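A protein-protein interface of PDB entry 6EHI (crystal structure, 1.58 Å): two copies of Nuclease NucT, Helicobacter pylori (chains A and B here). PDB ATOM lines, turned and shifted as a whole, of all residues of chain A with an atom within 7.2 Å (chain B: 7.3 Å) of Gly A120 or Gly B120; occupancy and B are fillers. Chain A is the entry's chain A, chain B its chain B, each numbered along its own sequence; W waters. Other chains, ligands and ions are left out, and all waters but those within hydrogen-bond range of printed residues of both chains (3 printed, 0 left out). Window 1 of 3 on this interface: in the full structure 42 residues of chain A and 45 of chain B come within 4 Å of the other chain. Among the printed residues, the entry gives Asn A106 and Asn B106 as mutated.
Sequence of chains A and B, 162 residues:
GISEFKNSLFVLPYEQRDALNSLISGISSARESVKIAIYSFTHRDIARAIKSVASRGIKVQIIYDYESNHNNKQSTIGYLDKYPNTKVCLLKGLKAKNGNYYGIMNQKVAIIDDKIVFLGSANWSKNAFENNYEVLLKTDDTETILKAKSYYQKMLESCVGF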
ATOM      1  N   ASN A 106      12.413   9.396 -16.171  1.00  0.00           N
ATOM      2  CA  ASN A 106      13.516  10.346 -15.819  1.00  0.00           C
ATOM      3  C   ASN A 106      14.235  10.045 -14.548  1.00  0.00           C
ATOM      4  O   ASN A 106      15.137  10.865 -14.137  1.00  0.00           O
ATOM      5  CB  ASN A 106      12.982  11.727 -15.684  1.00  0.00           C
ATOM      6  CG  ASN A 106      14.054  12.757 -15.877  1.00  0.00           C
ATOM      7  OD1 ASN A 106      14.843  12.718 -16.871  1.00  0.00           O
ATOM      8  ND2 ASN A 106      14.037  13.756 -14.986  1.00  0.00           N
ATOM      9  N   GLN A 107      13.968   8.966 -13.835  1.00  0.00           N
ATOM     10  CA  GLN A 107      14.752   8.623 -12.695  1.00  0.00           C
ATOM     11  C   GLN A 107      16.241   8.382 -12.951  1.00  0.00           C
ATOM     12  O   GLN A 107      16.628   8.012 -14.066  1.00  0.00           O
ATOM     13  CB  GLN A 107      14.221   7.338 -12.047  1.00  0.00           C
ATOM     14  CG  GLN A 107      12.797   7.527 -11.513  1.00  0.00           C
ATOM     15  CD  GLN A 107      12.254   6.280 -10.861  1.00  0.00           C
ATOM     16  OE1 GLN A 107      12.964   5.211 -10.755  1.00  0.00           O
ATOM     17  NE2 GLN A 107      11.002   6.366 -10.486  1.00  0.00           N
ATOM     18  N   LYS A 108      17.112   8.680 -11.953  1.00  0.00           N
ATOM     19  CA  LYS A 108      18.533   8.296 -12.015  1.00  0.00           C
ATOM     20  C   LYS A 108      18.798   7.674 -10.635  1.00  0.00           C
ATOM     21  O   LYS A 108      19.206   8.377  -9.718  1.00  0.00           O
ATOM     22  CB  LYS A 108      19.462   9.521 -12.232  1.00  0.00           C
ATOM     23  CG  LYS A 108      19.024  10.478 -13.344  1.00  0.00           C
ATOM     24  CD  LYS A 108      18.120  11.649 -12.972  1.00  0.00           C
ATOM     25  CE  LYS A 108      18.074  12.780 -14.005  1.00  0.00           C
ATOM     26  NZ  LYS A 108      17.365  12.379 -15.236  1.00  0.00           N
ATOM     27  N   VAL A 109      18.597   6.353 -10.561  1.00  0.00           N
ATOM     28  CA  VAL A 109      18.505   5.678  -9.286  1.00  0.00           C
ATOM     29  C   VAL A 109      19.308   4.412  -9.359  1.00  0.00           C
ATOM     30  O   VAL A 109      19.151   3.678 -10.332  1.00  0.00           O
ATOM     31  CB  VAL A 109      17.027   5.382  -9.007  1.00  0.00           C
ATOM     32  CG1 VAL A 109      16.864   4.436  -7.830  1.00  0.00           C
ATOM     33  CG2 VAL A 109      16.263   6.660  -8.756  1.00  0.00           C
ATOM     34  N   PHE A 118      21.231   5.377  -4.347  1.00  0.00           N
ATOM     35  CA  PHE A 118      21.780   6.590  -4.979  1.00  0.00           C
ATOM     36  C   PHE A 118      20.719   7.217  -5.774  1.00  0.00           C
ATOM     37  O   PHE A 118      19.988   6.578  -6.558  1.00  0.00           O
ATOM     38  CB  PHE A 118      22.956   6.270  -5.956  1.00  0.00           C
ATOM     39  CG  PHE A 118      24.167   5.679  -5.287  1.00  0.00           C
ATOM     40  CD1 PHE A 118      24.327   4.310  -5.096  1.00  0.00           C
ATOM     41  CD2 PHE A 118      25.238   6.498  -4.942  1.00  0.00           C
ATOM     42  CE1 PHE A 118      25.471   3.827  -4.555  1.00  0.00           C
ATOM     43  CE2 PHE A 118      26.394   6.001  -4.341  1.00  0.00           C
ATOM     44  CZ  PHE A 118      26.500   4.672  -4.142  1.00  0.00           C
ATOM     45  N   LEU A 119      20.453   8.472  -5.481  1.00  0.00           N
ATOM     46  CA  LEU A 119      19.509   9.211  -6.297  1.00  0.00           C
ATOM     47  C   LEU A 119      19.906  10.669  -6.475  1.00  0.00           C
ATOM     48  O   LEU A 119      20.861  11.086  -5.926  1.00  0.00           O
ATOM     49  CB  LEU A 119      18.062   9.076  -5.741  1.00  0.00           C
ATOM     50  CG  LEU A 119      17.779   9.626  -4.342  1.00  0.00           C
ATOM     51  CD1 LEU A 119      17.608  11.144  -4.310  1.00  0.00           C
ATOM     52  CD2 LEU A 119      16.534   9.049  -3.787  1.00  0.00           C
ATOM     53  N   GLY A 120      19.190  11.459  -7.268  1.00  0.00           N
ATOM     54  CA  GLY A 120      19.658  12.821  -7.543  1.00  0.00           C
ATOM     55  C   GLY A 120      19.389  13.204  -8.998  1.00  0.00           C
ATOM     56  O   GLY A 120      18.459  12.669  -9.639  1.00  0.00           O
ATOM     57  N   SER A 121      20.120  14.180  -9.483  1.00  0.00           N
ATOM     58  CA  SER A 121      19.833  14.812 -10.773  1.00  0.00           C
ATOM     59  C   SER A 121      20.666  14.296 -11.892  1.00  0.00           C
ATOM     60  O   SER A 121      20.355  14.618 -13.031  1.00  0.00           O
ATOM     61  CB  SER A 121      20.070  16.339 -10.657  1.00  0.00           C
ATOM     62  OG  SER A 121      21.419  16.685 -10.300  1.00  0.00           O
ATOM     63  N   ALA A 122      21.715  13.552 -11.584  1.00  0.00           N
ATOM     64  CA  ALA A 122      22.753  13.334 -12.592  1.00  0.00           C
ATOM     65  C   ALA A 122      22.401  12.099 -13.479  1.00  0.00           C
ATOM     66  O   ALA A 122      22.397  11.015 -12.990  1.00  0.00           O
ATOM     67  CB  ALA A 122      24.072  13.057 -11.932  1.00  0.00           C
ATOM     68  N   ASN A 123      22.330  12.351 -14.788  1.00  0.00           N
ATOM     69  CA  ASN A 123      22.358  11.281 -15.756  1.00  0.00           C
ATOM     70  C   ASN A 123      23.737  10.666 -15.760  1.00  0.00           C
ATOM     71  O   ASN A 123      24.731  11.281 -15.249  1.00  0.00           O
ATOM     72  CB  ASN A 123      21.946  11.785 -17.119  1.00  0.00           C
ATOM     73  CG  ASN A 123      20.435  12.152 -17.162  1.00  0.00           C
ATOM     74  OD1 ASN A 123      19.591  11.358 -16.674  1.00  0.00           O
ATOM     75  ND2 ASN A 123      20.076  13.289 -17.787  1.00  0.00           N
ATOM     76  N   GLU A 134      25.060  19.403 -10.562  1.00  0.00           N
ATOM     77  CA  GLU A 134      24.166  18.276 -10.297  1.00  0.00           C
ATOM     78  C   GLU A 134      24.164  18.096  -8.831  1.00  0.00           C
ATOM     79  O   GLU A 134      25.065  18.596  -8.110  1.00  0.00           O
ATOM     80  CB  GLU A 134      24.725  16.949 -10.901  1.00  0.00           C
ATOM     81  CG  GLU A 134      24.970  17.003 -12.377  1.00  0.00           C
ATOM     82  CD  GLU A 134      23.764  16.710 -13.255  1.00  0.00           C
ATOM     83  OE1 GLU A 134      22.593  16.647 -12.806  1.00  0.00           O
ATOM     84  OE2 GLU A 134      23.976  16.676 -14.483  1.00  0.00           O
ATOM     85  N   VAL A 135      23.283  17.256  -8.371  1.00  0.00           N
ATOM     86  CA  VAL A 135      23.410  16.678  -7.053  1.00  0.00           C
ATOM     87  C   VAL A 135      23.307  15.170  -7.123  1.00  0.00           C
ATOM     88  O   VAL A 135      22.437  14.589  -7.862  1.00  0.00           O
ATOM     89  CB  VAL A 135      22.473  17.262  -5.999  1.00  0.00           C
ATOM     90  CG1 VAL A 135      22.793  18.718  -5.712  1.00  0.00           C
ATOM     91  CG2 VAL A 135      21.015  17.092  -6.377  1.00  0.00           C
ATOM     92  N   LEU A 136      24.044  14.509  -6.232  1.00  0.00           N
ATOM     93  CA  LEU A 136      23.991  13.030  -6.117  1.00  0.00           C
ATOM     94  C   LEU A 136      23.896  12.720  -4.631  1.00  0.00           C
ATOM     95  O   LEU A 136      24.777  13.205  -3.835  1.00  0.00           O
ATOM     96  CB  LEU A 136      25.214  12.395  -6.741  1.00  0.00           C
ATOM     97  CG  LEU A 136      25.130  10.898  -6.971  1.00  0.00           C
ATOM     98  CD1 LEU A 136      25.970  10.540  -8.187  1.00  0.00           C
ATOM     99  CD2 LEU A 136      25.668  10.176  -5.785  1.00  0.00           C
ATOM    100  N   LEU A 137      22.868  12.014  -4.218  1.00  0.00           N
ATOM    101  CA  LEU A 137      22.675  11.620  -2.811  1.00  0.00           C
ATOM    102  C   LEU A 137      22.769  10.130  -2.636  1.00  0.00           C
ATOM    103  O   LEU A 137      22.113   9.369  -3.348  1.00  0.00           O
ATOM    104  CB  LEU A 137      21.350  12.097  -2.285  1.00  0.00           C
ATOM    105  CG  LEU A 137      21.243  11.790  -0.757  1.00  0.00           C
ATOM    106  CD1 LEU A 137      21.474  13.094  -0.056  1.00  0.00           C
ATOM    107  CD2 LEU A 137      19.972  11.177  -0.336  1.00  0.00           C
ATOM    108  N   ASN B 106      21.808  21.418 -13.924  1.00  0.00           N
ATOM    109  CA  ASN B 106      20.770  20.369 -14.011  1.00  0.00           C
ATOM    110  C   ASN B 106      20.209  20.024 -12.639  1.00  0.00           C
ATOM    111  O   ASN B 106      19.335  19.189 -12.535  1.00  0.00           O
ATOM    112  CB  ASN B 106      21.356  19.058 -14.534  1.00  0.00           C
ATOM    113  CG  ASN B 106      20.269  18.140 -15.114  1.00  0.00           C
ATOM    114  OD1 ASN B 106      19.331  18.605 -15.737  1.00  0.00           O
ATOM    115  ND2 ASN B 106      20.321  16.873 -14.746  1.00  0.00           N
ATOM    116  N   GLN B 107      20.617  20.745 -11.591  1.00  0.00           N
ATOM    117  CA  GLN B 107      20.081  20.434 -10.302  1.00  0.00           C
ATOM    118  C   GLN B 107      18.519  20.702 -10.257  1.00  0.00           C
ATOM    119  O   GLN B 107      17.992  21.533 -10.971  1.00  0.00           O
ATOM    120  CB  GLN B 107      20.786  21.262  -9.222  1.00  0.00           C
ATOM    121  CG  GLN B 107      22.180  20.841  -8.967  1.00  0.00           C
ATOM    122  CD  GLN B 107      22.832  21.843  -8.024  1.00  0.00           C
ATOM    123  OE1 GLN B 107      22.091  22.638  -7.392  1.00  0.00           O
ATOM    124  NE2 GLN B 107      24.141  21.663  -7.805  1.00  0.00           N
ATOM    125  N   LYS B 108      17.818  20.038  -9.361  1.00  0.00           N
ATOM    126  CA  LYS B 108      16.410  20.265  -9.043  1.00  0.00           C
ATOM    127  C   LYS B 108      16.337  20.222  -7.522  1.00  0.00           C
ATOM    128  O   LYS B 108      16.074  19.210  -6.853  1.00  0.00           O
ATOM    129  CB  LYS B 108      15.470  19.182  -9.652  1.00  0.00           C
ATOM    130  CG  LYS B 108      15.728  18.945 -11.137  1.00  0.00           C
ATOM    131  CD  LYS B 108      16.591  17.729 -11.377  1.00  0.00           C
ATOM    132  CE  LYS B 108      16.547  17.232 -12.840  1.00  0.00           C
ATOM    133  NZ  LYS B 108      16.940  18.117 -13.905  1.00  0.00           N
ATOM    134  N   VAL B 109      16.623  21.374  -6.911  1.00  0.00           N
ATOM    135  CA  VAL B 109      16.839  21.436  -5.473  1.00  0.00           C
ATOM    136  C   VAL B 109      16.107  22.635  -4.880  1.00  0.00           C
ATOM    137  O   VAL B 109      16.087  23.761  -5.429  1.00  0.00           O
ATOM    138  CB  VAL B 109      18.332  21.665  -5.192  1.00  0.00           C
ATOM    139  CG1 VAL B 109      18.597  21.957  -3.731  1.00  0.00           C
ATOM    140  CG2 VAL B 109      19.205  20.470  -5.600  1.00  0.00           C
ATOM    141  N   PHE B 118      14.802  19.515  -0.579  1.00  0.00           N
ATOM    142  CA  PHE B 118      14.149  18.646  -1.564  1.00  0.00           C
ATOM    143  C   PHE B 118      15.128  18.486  -2.719  1.00  0.00           C
ATOM    144  O   PHE B 118      15.701  19.472  -3.204  1.00  0.00           O
ATOM    145  CB  PHE B 118      12.899  19.313  -2.143  1.00  0.00           C
ATOM    146  CG  PHE B 118      11.753  19.455  -1.197  1.00  0.00           C
ATOM    147  CD1 PHE B 118      11.585  20.621  -0.420  1.00  0.00           C
ATOM    148  CD2 PHE B 118      10.809  18.497  -1.114  1.00  0.00           C
ATOM    149  CE1 PHE B 118      10.546  20.711   0.480  1.00  0.00           C
ATOM    150  CE2 PHE B 118       9.698  18.639  -0.232  1.00  0.00           C
ATOM    151  CZ  PHE B 118       9.597  19.735   0.586  1.00  0.00           C
ATOM    152  N   LEU B 119      15.325  17.259  -3.176  1.00  0.00           N
ATOM    153  CA  LEU B 119      16.170  16.979  -4.337  1.00  0.00           C
ATOM    154  C   LEU B 119      15.682  15.730  -5.025  1.00  0.00           C
ATOM    155  O   LEU B 119      14.789  15.033  -4.545  1.00  0.00           O
ATOM    156  CB  LEU B 119      17.623  16.812  -3.992  1.00  0.00           C
ATOM    157  CG  LEU B 119      18.012  15.837  -2.883  1.00  0.00           C
ATOM    158  CD1 LEU B 119      18.208  14.450  -3.525  1.00  0.00           C
ATOM    159  CD2 LEU B 119      19.311  16.133  -2.205  1.00  0.00           C
ATOM    160  N   GLY B 120      16.192  15.496  -6.175  1.00  0.00           N
ATOM    161  CA  GLY B 120      15.770  14.290  -6.901  1.00  0.00           C
ATOM    162  C   GLY B 120      15.852  14.541  -8.396  1.00  0.00           C
ATOM    163  O   GLY B 120      16.625  15.377  -8.874  1.00  0.00           O
ATOM    164  N   SER B 121      15.011  13.796  -9.137  1.00  0.00           N
ATOM    165  CA  SER B 121      15.094  13.856 -10.599  1.00  0.00           C
ATOM    166  C   SER B 121      14.088  14.770 -11.270  1.00  0.00           C
ATOM    167  O   SER B 121      14.265  15.040 -12.468  1.00  0.00           O
ATOM    168  CB  SER B 121      14.882  12.449 -11.165  1.00  0.00           C
ATOM    169  OG  SER B 121      13.560  12.048 -10.858  1.00  0.00           O
ATOM    170  N   ALA B 122      13.156  15.330 -10.551  1.00  0.00           N
ATOM    171  CA  ALA B 122      12.033  15.996 -11.169  1.00  0.00           C
ATOM    172  C   ALA B 122      12.289  17.434 -11.521  1.00  0.00           C
ATOM    173  O   ALA B 122      12.369  18.242 -10.623  1.00  0.00           O
ATOM    174  CB  ALA B 122      10.784  15.858 -10.323  1.00  0.00           C
ATOM    175  N   ASN B 123      12.301  17.767 -12.817  1.00  0.00           N
ATOM    176  CA  ASN B 123      12.076  19.172 -13.178  1.00  0.00           C
ATOM    177  C   ASN B 123      10.685  19.682 -12.697  1.00  0.00           C
ATOM    178  O   ASN B 123       9.802  18.885 -12.377  1.00  0.00           O
ATOM    179  CB  ASN B 123      12.304  19.399 -14.647  1.00  0.00           C
ATOM    180  CG  ASN B 123      13.684  19.166 -15.019  1.00  0.00           C
ATOM    181  OD1 ASN B 123      14.603  19.783 -14.405  1.00  0.00           O
ATOM    182  ND2 ASN B 123      13.918  18.383 -16.073  1.00  0.00           N
ATOM    183  N   GLU B 134       9.885   9.489 -11.822  1.00  0.00           N
ATOM    184  CA  GLU B 134      10.777  10.459 -11.156  1.00  0.00           C
ATOM    185  C   GLU B 134      10.940   9.994  -9.764  1.00  0.00           C
ATOM    186  O   GLU B 134      10.085   9.175  -9.282  1.00  0.00           O
ATOM    187  CB  GLU B 134      10.158  11.933 -11.019  1.00  0.00           C
ATOM    188  CG  GLU B 134       9.650  12.631 -12.248  1.00  0.00           C
ATOM    189  CD  GLU B 134      10.743  13.184 -13.188  1.00  0.00           C
ATOM    190  OE1 GLU B 134      11.958  13.060 -12.847  1.00  0.00           O
ATOM    191  OE2 GLU B 134      10.362  13.716 -14.251  1.00  0.00           O
ATOM    192  N   VAL B 135      11.920  10.599  -9.060  1.00  0.00           N
ATOM    193  CA  VAL B 135      12.031  10.448  -7.644  1.00  0.00           C
ATOM    194  C   VAL B 135      12.202  11.823  -7.027  1.00  0.00           C
ATOM    195  O   VAL B 135      12.863  12.706  -7.634  1.00  0.00           O
ATOM    196  CB  VAL B 135      13.173   9.580  -7.191  1.00  0.00           C
ATOM    197  CG1 VAL B 135      12.822   8.104  -7.400  1.00  0.00           C
ATOM    198  CG2 VAL B 135      14.472   9.968  -7.771  1.00  0.00           C
ATOM    199  N   LEU B 136      11.539  12.051  -5.911  1.00  0.00           N
ATOM    200  CA  LEU B 136      11.687  13.307  -5.108  1.00  0.00           C
ATOM    201  C   LEU B 136      11.984  12.873  -3.705  1.00  0.00           C
ATOM    202  O   LEU B 136      11.259  12.076  -3.148  1.00  0.00           O
ATOM    203  CB  LEU B 136      10.457  14.160  -5.234  1.00  0.00           C
ATOM    204  CG  LEU B 136      10.340  15.565  -4.674  1.00  0.00           C
ATOM    205  CD1 LEU B 136       9.739  16.432  -5.780  1.00  0.00           C
ATOM    206  CD2 LEU B 136       9.361  15.559  -3.545  1.00  0.00           C
ATOM    207  N   LEU B 137      13.101  13.332  -3.152  1.00  0.00           N
ATOM    208  CA  LEU B 137      13.442  13.114  -1.785  1.00  0.00           C
ATOM    209  C   LEU B 137      13.345  14.442  -0.977  1.00  0.00           C
ATOM    210  O   LEU B 137      14.004  15.389  -1.308  1.00  0.00           O
ATOM    211  CB  LEU B 137      14.827  12.585  -1.662  1.00  0.00           C
ATOM    212  CG  LEU B 137      15.190  12.195  -0.205  1.00  0.00           C
ATOM    213  CD1 LEU B 137      14.706  10.836   0.125  1.00  0.00           C
ATOM    214  CD2 LEU B 137      16.666  12.199  -0.044  1.00  0.00           C
HETATM  215  O   HOH W   1      13.188  16.026 -17.411  1.00  0.00           O
HETATM  216  O   HOH W   2      11.645  16.001 -15.058  1.00  0.00           O
HETATM  217  O   HOH W   3      22.660  14.934 -16.049  1.00  0.00           O
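O of Ser B121 sits at hydrogen-bond distance from ND2 of Asn A106 (2.8 Å). The side-chain amide nitrogen of Asn A106 lies within hydrogen-bond range of the side-chain carboxylate of Glu B134 (3.1 Å). O of Glu B134 is in hydrogen-bond range of NE2 of Gln A107, 3.2 Å away. The side-chain amide nitrogen (ND2) of Asn B106 is in hydrogen-bond range of the backbone carbonyl oxygen (O) of Ser A121, 2.8 Å away. The side-chain carboxylate of Glu A134 is in hydrogen-bond range of the side-chain amide nitrogen of Asn B106 (3.0 Å). O of Glu A134 lies within hydrogen-bond range of NE2 of Gln B107 (3.2 Å). O of Gly B120 lies close to O of Gly A120, 3.4 Å away.
The side-chain amino group (NZ) of Lys A108 lies within hydrogen-bond range of the side-chain amide oxygen (OD1) of Asn A123. The backbone carbonyl oxygen (O) of Leu A119 sits at hydrogen-bond distance from the backbone NH (N) of Leu A137, at 2.8 Å. OG of Ser A121 sits at hydrogen-bond distance from N of Val A135 (2.7 Å). NZ of Lys B108 is in hydrogen-bond range of O of Asn B106 (3.0 Å). NZ of Lys B108 is in hydrogen-bond range of OD1 of Asn B123 (2.9 Å). The backbone NH (N) of Ala B122 sits close to the side-chain carboxylate (OE1) of Glu B134, at 3.4 Å.
Val B135 touches Gln A107. Ser B121 touches Lys A108 (CB to CD, 3.8 Å). Val A109 touches Val B135 (CG2 to CG2, 3.9 Å). Leu B119 touches Leu A119 (CD1 to CD1, 3.5 Å). O of Gly A120 touches N of Ser B121, 3.7 Å away. OG of Ser A121 touches CA of Gln B107 (3.98 Å). Lys B108 touches Ser A121. Ser A121 touches Gly B120. Val A135 touches Gln B107. Leu A137 touches Leu B137.
Of chain B, only Gly B120 and Ser B121 come within 4 Å of Gly A120. Of the printed residues of chain B, Val A135 touches Gln B107 and Val B109. Leu A136 touches none of the printed residues of chain B. Of the printed residues of chain B, Leu A137 touches Leu B137 (3.5 Å). Gly B120 touches two residues of chain A. Of the printed residues of chain A, Leu B137 touches Leu A137. The nearest residue of chain B that does not touch Gly A120 is Leu B119 (4.6 Å).
Hydrophobic or aromatic side chains of chain A that line the printed part of chain B: Val A109, Leu A119, Val A135 and Leu A137. Along chain A the printed residues that touch a printed residue of chain B span positions 106 to 137. Hydrophobic or aromatic side chains of chain B that line the printed part of chain A: Val B109, Leu B119, Val B135 and Leu B137.
Asn A106 touches Ser B121, and with the chains exchanged Ser A121 touches Asn B106. Val A109 touches Val B135, and with the chains exchanged Val A135 touches Val B109. Leu B119 touches its own counterpart, Leu A119. Gly A120 touches Ser B121, and with the chains exchanged Ser A121 touches Gly B120. Positions printed for both chains: 106, 107, 108, 109, 118, 119, 120, 121, 122, 123, 134, 135, 136 and 137.
Water W3 lies within hydrogen-bond range of OE2 of Glu A134 (2.7 Å), N of Asn A123 (2.9 Å) and ND2 of Asn B106 (3.3 Å). Water W2 lies within hydrogen-bond range of the side-chain carboxylate (OE2) of Glu B134, the backbone NH (N) of Asn B123 and the side-chain amide nitrogen (ND2) of Asn A106. Water W1 bridges ND2 of Asn B123 (2.8 Å) and ND2 of Asn A106 (3.4 Å).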
